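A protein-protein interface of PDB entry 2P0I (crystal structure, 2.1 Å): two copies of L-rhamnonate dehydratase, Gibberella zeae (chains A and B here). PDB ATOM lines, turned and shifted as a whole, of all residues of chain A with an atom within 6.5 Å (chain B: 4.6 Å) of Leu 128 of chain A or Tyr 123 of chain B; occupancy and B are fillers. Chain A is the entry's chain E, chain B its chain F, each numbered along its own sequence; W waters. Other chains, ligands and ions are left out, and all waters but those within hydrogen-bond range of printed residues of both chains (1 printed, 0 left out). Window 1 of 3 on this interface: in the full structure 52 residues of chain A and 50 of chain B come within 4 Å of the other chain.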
ATOM      1  N   GLY A  60     -30.504  -4.263   5.168  1.00  0.00           N
ATOM      2  CA  GLY A  60     -29.658  -4.606   6.308  1.00  0.00           C
ATOM      3  C   GLY A  60     -28.236  -4.098   6.189  1.00  0.00           C
ATOM      4  O   GLY A  60     -27.284  -4.862   6.349  1.00  0.00           O
ATOM      5  N   VAL A  63     -26.695  -4.353   9.758  1.00  0.00           N
ATOM      6  CA  VAL A  63     -26.928  -5.699  10.262  1.00  0.00           C
ATOM      7  C   VAL A  63     -25.812  -6.227  11.169  1.00  0.00           C
ATOM      8  O   VAL A  63     -26.084  -6.976  12.102  1.00  0.00           O
ATOM      9  CB  VAL A  63     -27.291  -6.698   9.124  1.00  0.00           C
ATOM     10  CG1 VAL A  63     -26.049  -7.245   8.405  1.00  0.00           C
ATOM     11  CG2 VAL A  63     -28.139  -7.819   9.661  1.00  0.00           C
ATOM     12  N   LEU A  64     -24.575  -5.802  10.913  1.00  0.00           N
ATOM     13  CA  LEU A  64     -23.413  -6.319  11.634  1.00  0.00           C
ATOM     14  C   LEU A  64     -23.224  -5.618  12.975  1.00  0.00           C
ATOM     15  O   LEU A  64     -22.958  -6.268  13.990  1.00  0.00           O
ATOM     16  CB  LEU A  64     -22.139  -6.195  10.789  1.00  0.00           C
ATOM     17  CG  LEU A  64     -22.033  -6.990   9.481  1.00  0.00           C
ATOM     18  CD1 LEU A  64     -20.699  -6.690   8.785  1.00  0.00           C
ATOM     19  CD2 LEU A  64     -22.206  -8.495   9.710  1.00  0.00           C
ATOM     20  N   PHE A  84     -16.733  -1.849  12.265  1.00  0.00           N
ATOM     21  CA  PHE A  84     -17.932  -2.638  12.015  1.00  0.00           C
ATOM     22  C   PHE A  84     -17.623  -4.138  11.986  1.00  0.00           C
ATOM     23  O   PHE A  84     -16.526  -4.548  11.614  1.00  0.00           O
ATOM     24  CB  PHE A  84     -18.604  -2.192  10.712  1.00  0.00           C
ATOM     25  CG  PHE A  84     -19.251  -0.828  10.791  1.00  0.00           C
ATOM     26  CD1 PHE A  84     -20.247  -0.560  11.734  1.00  0.00           C
ATOM     27  CD2 PHE A  84     -18.878   0.185   9.911  1.00  0.00           C
ATOM     28  CE1 PHE A  84     -20.854   0.703  11.806  1.00  0.00           C
ATOM     29  CE2 PHE A  84     -19.481   1.452   9.973  1.00  0.00           C
ATOM     30  CZ  PHE A  84     -20.470   1.710  10.923  1.00  0.00           C
ATOM     31  N   GLY A  85     -18.596  -4.944  12.397  1.00  0.00           N
ATOM     32  CA  GLY A  85     -18.456  -6.391  12.406  1.00  0.00           C
ATOM     33  C   GLY A  85     -19.283  -7.035  13.501  1.00  0.00           C
ATOM     34  O   GLY A  85     -19.971  -8.031  13.268  1.00  0.00           O
ATOM     35  N   GLY A  86     -19.199  -6.471  14.702  1.00  0.00           N
ATOM     36  CA  GLY A  86     -20.106  -6.811  15.792  1.00  0.00           C
ATOM     37  C   GLY A  86     -19.848  -8.186  16.378  1.00  0.00           C
ATOM     38  O   GLY A  86     -18.696  -8.590  16.514  1.00  0.00           O
ATOM     39  N   PRO A  88     -20.372 -11.551  15.198  1.00  0.00           N
ATOM     40  CA  PRO A  88     -19.601 -12.622  14.542  1.00  0.00           C
ATOM     41  C   PRO A  88     -18.107 -12.299  14.343  1.00  0.00           C
ATOM     42  O   PRO A  88     -17.285 -13.215  14.249  1.00  0.00           O
ATOM     43  CB  PRO A  88     -20.299 -12.771  13.188  1.00  0.00           C
ATOM     44  CG  PRO A  88     -20.871 -11.427  12.912  1.00  0.00           C
ATOM     45  CD  PRO A  88     -21.311 -10.915  14.247  1.00  0.00           C
ATOM     46  N   ALA A  89     -17.776 -11.009  14.287  1.00  0.00           N
ATOM     47  CA  ALA A  89     -16.396 -10.533  14.344  1.00  0.00           C
ATOM     48  C   ALA A  89     -15.694 -10.881  15.655  1.00  0.00           C
ATOM     49  O   ALA A  89     -14.613 -11.475  15.640  1.00  0.00           O
ATOM     50  CB  ALA A  89     -16.349  -9.049  14.102  1.00  0.00           C
ATOM     51  N   LEU A  92     -14.871 -14.560  15.984  1.00  0.00           N
ATOM     52  CA  LEU A  92     -13.685 -14.962  15.225  1.00  0.00           C
ATOM     53  C   LEU A  92     -12.369 -14.529  15.870  1.00  0.00           C
ATOM     54  O   LEU A  92     -11.380 -15.249  15.749  1.00  0.00           O
ATOM     55  CB  LEU A  92     -13.766 -14.486  13.764  1.00  0.00           C
ATOM     56  CG  LEU A  92     -14.789 -15.159  12.832  1.00  0.00           C
ATOM     57  CD1 LEU A  92     -15.069 -14.273  11.619  1.00  0.00           C
ATOM     58  CD2 LEU A  92     -14.353 -16.566  12.381  1.00  0.00           C
ATOM     59  N   LYS A 126     -11.731 -12.191   1.352  1.00  0.00           N
ATOM     60  CA  LYS A 126     -12.589 -11.019   1.178  1.00  0.00           C
ATOM     61  C   LYS A 126     -13.628 -10.962   2.298  1.00  0.00           C
ATOM     62  O   LYS A 126     -13.875 -11.965   2.980  1.00  0.00           O
ATOM     63  CB  LYS A 126     -13.281 -11.041  -0.196  1.00  0.00           C
ATOM     64  CG  LYS A 126     -12.345 -11.315  -1.378  1.00  0.00           C
ATOM     65  CD  LYS A 126     -12.425 -10.254  -2.464  1.00  0.00           C
ATOM     66  CE  LYS A 126     -11.414 -10.541  -3.575  1.00  0.00           C
ATOM     67  NZ  LYS A 126     -10.134  -9.786  -3.400  1.00  0.00           N
ATOM     68  N   GLY A 127     -14.207  -9.781   2.495  1.00  0.00           N
ATOM     69  CA  GLY A 127     -15.381  -9.605   3.344  1.00  0.00           C
ATOM     70  C   GLY A 127     -15.129  -9.627   4.840  1.00  0.00           C
ATOM     71  O   GLY A 127     -14.190  -8.996   5.329  1.00  0.00           O
ATOM     72  N   LEU A 128     -15.976 -10.366   5.560  1.00  0.00           N
ATOM     73  CA  LEU A 128     -16.059 -10.309   7.026  1.00  0.00           C
ATOM     74  C   LEU A 128     -14.807 -10.704   7.833  1.00  0.00           C
ATOM     75  O   LEU A 128     -14.433  -9.960   8.741  1.00  0.00           O
ATOM     76  CB  LEU A 128     -17.326 -11.022   7.539  1.00  0.00           C
ATOM     77  CG  LEU A 128     -17.725 -10.985   9.021  1.00  0.00           C
ATOM     78  CD1 LEU A 128     -17.744  -9.566   9.591  1.00  0.00           C
ATOM     79  CD2 LEU A 128     -19.094 -11.648   9.192  1.00  0.00           C
ATOM     80  N   PRO A 129     -14.140 -11.841   7.503  1.00  0.00           N
ATOM     81  CA  PRO A 129     -12.964 -12.227   8.310  1.00  0.00           C
ATOM     82  C   PRO A 129     -11.810 -11.229   8.188  1.00  0.00           C
ATOM     83  O   PRO A 129     -11.020 -11.074   9.122  1.00  0.00           O
ATOM     84  CB  PRO A 129     -12.546 -13.576   7.706  1.00  0.00           C
ATOM     85  CG  PRO A 129     -13.725 -14.033   6.926  1.00  0.00           C
ATOM     86  CD  PRO A 129     -14.371 -12.810   6.417  1.00  0.00           C
ATOM     87  N   ILE A 130     -11.753 -10.549   7.046  1.00  0.00           N
ATOM     88  CA  ILE A 130     -10.726  -9.557   6.740  1.00  0.00           C
ATOM     89  C   ILE A 130     -10.929  -8.267   7.541  1.00  0.00           C
ATOM     90  O   ILE A 130      -9.955  -7.636   7.973  1.00  0.00           O
ATOM     91  CB  ILE A 130     -10.667  -9.263   5.209  1.00  0.00           C
ATOM     92  CG1 ILE A 130     -10.650 -10.566   4.389  1.00  0.00           C
ATOM     93  CG2 ILE A 130      -9.434  -8.461   4.858  1.00  0.00           C
ATOM     94  CD1 ILE A 130      -9.534 -11.574   4.755  1.00  0.00           C
ATOM     95  N   ALA A 131     -12.194  -7.902   7.755  1.00  0.00           N
ATOM     96  CA  ALA A 131     -12.567  -6.862   8.717  1.00  0.00           C
ATOM     97  C   ALA A 131     -12.083  -7.146  10.148  1.00  0.00           C
ATOM     98  O   ALA A 131     -11.632  -6.238  10.850  1.00  0.00           O
ATOM     99  CB  ALA A 131     -14.063  -6.634   8.692  1.00  0.00           C
ATOM    100  N   VAL A 132     -12.162  -8.405  10.559  1.00  0.00           N
ATOM    101  CA  VAL A 132     -11.626  -8.837  11.850  1.00  0.00           C
ATOM    102  C   VAL A 132     -10.106  -8.704  11.887  1.00  0.00           C
ATOM    103  O   VAL A 132      -9.546  -8.264  12.894  1.00  0.00           O
ATOM    104  CB  VAL A 132     -12.045 -10.283  12.191  1.00  0.00           C
ATOM    105  CG1 VAL A 132     -11.720 -10.612  13.634  1.00  0.00           C
ATOM    106  CG2 VAL A 132     -13.526 -10.486  11.925  1.00  0.00           C
ATOM    107  N   ILE A 133      -9.451  -9.060  10.780  1.00  0.00           N
ATOM    108  CA  ILE A 133      -8.008  -8.866  10.638  1.00  0.00           C
ATOM    109  C   ILE A 133      -7.595  -7.398  10.751  1.00  0.00           C
ATOM    110  O   ILE A 133      -6.607  -7.074  11.432  1.00  0.00           O
ATOM    111  CB  ILE A 133      -7.407  -9.577   9.371  1.00  0.00           C
ATOM    112  CG1 ILE A 133      -7.682 -11.093   9.407  1.00  0.00           C
ATOM    113  CG2 ILE A 133      -5.895  -9.367   9.297  1.00  0.00           C
ATOM    114  CD1 ILE A 133      -7.423 -11.833   8.091  1.00  0.00           C
ATOM    115  N   HIS A 276     -15.093  -1.565  -1.262  1.00  0.00           N
ATOM    116  CA  HIS A 276     -15.505  -2.924  -0.968  1.00  0.00           C
ATOM    117  C   HIS A 276     -14.582  -3.947  -1.607  1.00  0.00           C
ATOM    118  O   HIS A 276     -15.007  -5.033  -2.018  1.00  0.00           O
ATOM    119  CB  HIS A 276     -16.972  -3.114  -1.350  1.00  0.00           C
ATOM    120  CG  HIS A 276     -17.882  -2.159  -0.646  1.00  0.00           C
ATOM    121  ND1 HIS A 276     -18.269  -0.955  -1.197  1.00  0.00           N
ATOM    122  CD2 HIS A 276     -18.440  -2.205   0.587  1.00  0.00           C
ATOM    123  CE1 HIS A 276     -19.047  -0.314  -0.344  1.00  0.00           C
ATOM    124  NE2 HIS A 276     -19.166  -1.049   0.747  1.00  0.00           N
ATOM    125  N   TYR A 278     -10.445  -5.783  -1.014  1.00  0.00           N
ATOM    126  CA  TYR A 278      -9.738  -6.392   0.121  1.00  0.00           C
ATOM    127  C   TYR A 278      -8.390  -6.959  -0.341  1.00  0.00           C
ATOM    128  O   TYR A 278      -8.304  -7.555  -1.420  1.00  0.00           O
ATOM    129  CB  TYR A 278     -10.555  -7.547   0.733  1.00  0.00           C
ATOM    130  CG  TYR A 278     -12.011  -7.238   1.008  1.00  0.00           C
ATOM    131  CD1 TYR A 278     -12.408  -6.706   2.233  1.00  0.00           C
ATOM    132  CD2 TYR A 278     -12.996  -7.474   0.039  1.00  0.00           C
ATOM    133  CE1 TYR A 278     -13.741  -6.417   2.487  1.00  0.00           C
ATOM    134  CE2 TYR A 278     -14.330  -7.182   0.284  1.00  0.00           C
ATOM    135  CZ  TYR A 278     -14.698  -6.650   1.509  1.00  0.00           C
ATOM    136  OH  TYR A 278     -16.020  -6.370   1.763  1.00  0.00           O
ATOM    137  N   TRP A 301     -11.439  -2.499   6.743  1.00  0.00           N
ATOM    138  CA  TRP A 301     -12.142  -3.498   5.940  1.00  0.00           C
ATOM    139  C   TRP A 301     -11.139  -4.360   5.149  1.00  0.00           C
ATOM    140  O   TRP A 301     -11.246  -5.592   5.128  1.00  0.00           O
ATOM    141  CB  TRP A 301     -13.133  -2.782   5.006  1.00  0.00           C
ATOM    142  CG  TRP A 301     -14.495  -3.417   4.837  1.00  0.00           C
ATOM    143  CD1 TRP A 301     -15.086  -3.762   3.655  1.00  0.00           C
ATOM    144  CD2 TRP A 301     -15.445  -3.746   5.868  1.00  0.00           C
ATOM    145  NE1 TRP A 301     -16.324  -4.311   3.880  1.00  0.00           N
ATOM    146  CE2 TRP A 301     -16.573  -4.311   5.228  1.00  0.00           C
ATOM    147  CE3 TRP A 301     -15.452  -3.624   7.265  1.00  0.00           C
ATOM    148  CZ2 TRP A 301     -17.695  -4.757   5.938  1.00  0.00           C
ATOM    149  CZ3 TRP A 301     -16.567  -4.072   7.970  1.00  0.00           C
ATOM    150  CH2 TRP A 301     -17.671  -4.633   7.304  1.00  0.00           C
ATOM    151  N   LEU B  92     -25.758 -14.844  11.206  1.00  0.00           N
ATOM    152  CA  LEU B  92     -26.150 -14.251   9.928  1.00  0.00           C
ATOM    153  C   LEU B  92     -27.496 -14.726   9.365  1.00  0.00           C
ATOM    154  O   LEU B  92     -28.225 -13.928   8.767  1.00  0.00           O
ATOM    155  CB  LEU B  92     -25.039 -14.438   8.887  1.00  0.00           C
ATOM    156  CG  LEU B  92     -23.757 -13.629   9.108  1.00  0.00           C
ATOM    157  CD1 LEU B  92     -22.591 -14.253   8.348  1.00  0.00           C
ATOM    158  CD2 LEU B  92     -23.962 -12.167   8.719  1.00  0.00           C
ATOM    159  N   HIS B  96     -29.590 -11.345   9.238  1.00  0.00           N
ATOM    160  CA  HIS B  96     -29.655 -10.778   7.892  1.00  0.00           C
ATOM    161  C   HIS B  96     -30.676 -11.440   6.981  1.00  0.00           C
ATOM    162  O   HIS B  96     -31.485 -10.760   6.357  1.00  0.00           O
ATOM    163  CB  HIS B  96     -28.274 -10.740   7.220  1.00  0.00           C
ATOM    164  CG  HIS B  96     -28.134  -9.667   6.180  1.00  0.00           C
ATOM    165  ND1 HIS B  96     -26.924  -9.340   5.610  1.00  0.00           N
ATOM    166  CD2 HIS B  96     -29.048  -8.843   5.612  1.00  0.00           C
ATOM    167  CE1 HIS B  96     -27.098  -8.369   4.732  1.00  0.00           C
ATOM    168  NE2 HIS B  96     -28.377  -8.048   4.717  1.00  0.00           N
ATOM    169  N   PHE B  97     -30.629 -12.760   6.887  1.00  0.00           N
ATOM    170  CA  PHE B  97     -31.184 -13.437   5.719  1.00  0.00           C
ATOM    171  C   PHE B  97     -32.625 -13.906   5.909  1.00  0.00           C
ATOM    172  O   PHE B  97     -33.352 -14.098   4.929  1.00  0.00           O
ATOM    173  CB  PHE B  97     -30.282 -14.595   5.300  1.00  0.00           C
ATOM    174  CG  PHE B  97     -28.933 -14.163   4.804  1.00  0.00           C
ATOM    175  CD1 PHE B  97     -28.810 -13.139   3.867  1.00  0.00           C
ATOM    176  CD2 PHE B  97     -27.783 -14.800   5.256  1.00  0.00           C
ATOM    177  CE1 PHE B  97     -27.556 -12.745   3.401  1.00  0.00           C
ATOM    178  CE2 PHE B  97     -26.525 -14.416   4.796  1.00  0.00           C
ATOM    179  CZ  PHE B  97     -26.411 -13.388   3.870  1.00  0.00           C
ATOM    180  N   SER B 120     -25.950  -8.497   1.063  1.00  0.00           N
ATOM    181  CA  SER B 120     -24.780  -8.802   1.867  1.00  0.00           C
ATOM    182  C   SER B 120     -23.492  -8.449   1.141  1.00  0.00           C
ATOM    183  O   SER B 120     -22.404  -8.782   1.606  1.00  0.00           O
ATOM    184  CB  SER B 120     -24.773 -10.281   2.252  1.00  0.00           C
ATOM    185  OG  SER B 120     -24.535 -11.096   1.123  1.00  0.00           O
ATOM    186  N   MET B 121     -23.627  -7.767   0.008  1.00  0.00           N
ATOM    187  CA  MET B 121     -22.505  -7.430  -0.865  1.00  0.00           C
ATOM    188  C   MET B 121     -21.417  -6.612  -0.161  1.00  0.00           C
ATOM    189  O   MET B 121     -20.227  -6.790  -0.440  1.00  0.00           O
ATOM    190  CB  MET B 121     -23.016  -6.676  -2.091  1.00  0.00           C
ATOM    191  CG  MET B 121     -22.104  -6.731  -3.292  1.00  0.00           C
ATOM    192  SD  MET B 121     -22.929  -5.908  -4.849  1.00  0.00           S
ATOM    193  CE  MET B 121     -23.643  -7.508  -5.670  1.00  0.00           C
ATOM    194  N   PHE B 122     -21.831  -5.734   0.754  1.00  0.00           N
ATOM    195  CA  PHE B 122     -20.907  -4.858   1.474  1.00  0.00           C
ATOM    196  C   PHE B 122     -19.933  -5.569   2.423  1.00  0.00           C
ATOM    197  O   PHE B 122     -18.858  -5.045   2.712  1.00  0.00           O
ATOM    198  CB  PHE B 122     -21.648  -3.704   2.168  1.00  0.00           C
ATOM    199  CG  PHE B 122     -22.470  -4.117   3.369  1.00  0.00           C
ATOM    200  CD1 PHE B 122     -21.969  -3.947   4.664  1.00  0.00           C
ATOM    201  CD2 PHE B 122     -23.755  -4.637   3.214  1.00  0.00           C
ATOM    202  CE1 PHE B 122     -22.726  -4.309   5.782  1.00  0.00           C
ATOM    203  CE2 PHE B 122     -24.521  -5.006   4.328  1.00  0.00           C
ATOM    204  CZ  PHE B 122     -24.008  -4.836   5.612  1.00  0.00           C
ATOM    205  N   TYR B 123     -20.310  -6.754   2.899  1.00  0.00           N
ATOM    206  CA  TYR B 123     -19.427  -7.559   3.745  1.00  0.00           C
ATOM    207  C   TYR B 123     -19.173  -8.959   3.196  1.00  0.00           C
ATOM    208  O   TYR B 123     -18.505  -9.770   3.844  1.00  0.00           O
ATOM    209  CB  TYR B 123     -19.952  -7.622   5.185  1.00  0.00           C
ATOM    210  CG  TYR B 123     -21.239  -8.403   5.352  1.00  0.00           C
ATOM    211  CD1 TYR B 123     -21.218  -9.744   5.719  1.00  0.00           C
ATOM    212  CD2 TYR B 123     -22.473  -7.797   5.154  1.00  0.00           C
ATOM    213  CE1 TYR B 123     -22.385 -10.463   5.863  1.00  0.00           C
ATOM    214  CE2 TYR B 123     -23.654  -8.506   5.307  1.00  0.00           C
ATOM    215  CZ  TYR B 123     -23.600  -9.844   5.662  1.00  0.00           C
ATOM    216  OH  TYR B 123     -24.751 -10.577   5.817  1.00  0.00           O
ATOM    217  N   GLY B 124     -19.709  -9.245   2.011  1.00  0.00           N
ATOM    218  CA  GLY B 124     -19.669 -10.599   1.460  1.00  0.00           C
ATOM    219  C   GLY B 124     -18.948 -10.681   0.133  1.00  0.00           C
ATOM    220  O   GLY B 124     -17.740 -10.426   0.064  1.00  0.00           O
ATOM    221  N   PRO B 129     -20.042 -15.253   4.451  1.00  0.00           N
ATOM    222  CA  PRO B 129     -21.466 -14.961   4.218  1.00  0.00           C
ATOM    223  C   PRO B 129     -22.073 -15.715   3.026  1.00  0.00           C
ATOM    224  O   PRO B 129     -23.287 -15.907   2.975  1.00  0.00           O
ATOM    225  CB  PRO B 129     -21.478 -13.454   3.921  1.00  0.00           C
ATOM    226  CG  PRO B 129     -20.183 -12.947   4.417  1.00  0.00           C
ATOM    227  CD  PRO B 129     -19.214 -14.052   4.240  1.00  0.00           C
HETATM  228  O   HOH W   1     -17.533  -7.207  -0.260  1.00  0.00           O
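2 positions are printed for both chains. Of the 10 pairs that touch across the chains among the printed residues, none has its exchanged pair printed and touching as well.
Printed residues of chain B that touch a printed residue of chain A: His 96, Phe 122 and Tyr 123. Hydrophobic or aromatic side chains of chain B within 4 Å of the printed part of chain A: His 96, Phe 122 and Tyr 123. Of the 20 printed residues of chain A, 8 touch a printed residue of chain B. Printed residues of chain A that touch a printed residue of chain B: Gly 60, Val 63, Leu 64, Gly 127, Leu 128, His 276, Tyr 278 and Trp 301. Among the printed residues, no Asp or Glu carboxylate lies within 4 Å of a Lys or Arg side-chain nitrogen of the other chain.
Among the printed residues, pairs that only touch across the chains: Gly 127 of chain A with Tyr 123 of chain B, Gly 60 of chain A with Phe 122 of chain B, His 276 of chain A with Phe 122 of chain B, Val 63 of chain A with His 96 of chain B, Trp 301 of chain A with Tyr 123 of chain B, Gly 60 of chain A with His 96 of chain B and Leu 64 of chain A with Tyr 123 of chain B.
Printed residues of chain B within 4 Å of Leu 64 of chain A: Tyr 123 (3.8 Å). Leu 92 of chain A touches none of the printed residues of chain B. Of the printed residues of chain B, Gly 127 of chain A touches Tyr 123. Leu 128 of chain A touches just one residue of chain B: Tyr 123 (3.1 Å). Printed residues of chain B within 4 Å of His 276 of chain A: Phe 122 (3.6 Å). Of the printed residues of chain B, Tyr 278 of chain A touches Phe 122 (3.3 Å). Phe 97 of chain B touches none of the printed residues of chain A. Of chain A, only Leu 64, Gly 127, Leu 128 and Trp 301 come within 4 Å of Tyr 123 of chain B. The nearest residue of chain B that does not touch Leu 128 of chain A is Leu 92 of chain B (4.4 Å). The nearest printed residue of chain A that does not touch Tyr 123 of chain B is Val 63 of chain A (4.1 Å).
N of Leu 128 of chain A is in hydrogen-bond range of O of Tyr 123 of chain B, 3.1 Å away. OH of Tyr 278 of chain A is in hydrogen-bond range of O of Phe 122 of chain B, 3.3 Å away. The backbone carbonyl oxygen (O) of Phe 122 of chain B lies within hydrogen-bond range of the indole nitrogen (NE1) of Trp 301 of chain A (2.9 Å).
Water W1 lies within hydrogen-bond range of OH of Tyr 278 of chain A, O of Met 121 of chain B and O of Gly 124 of chain B.
O of Tyr 278 of chain A sits at hydrogen-bond distance from NZ of Lys 126 of chain A (3.5 Å). The side-chain hydroxyl (OH) of Tyr 278 of chain A is in hydrogen-bond range of the indole nitrogen (NE1) of Trp 301 of chain A, 3.0 Å away. A ring nitrogen (ND1) of His 96 of chain B sits at hydrogen-bond distance from the side-chain hydroxyl (OH) of Tyr 123 of chain B (2.5 Å).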
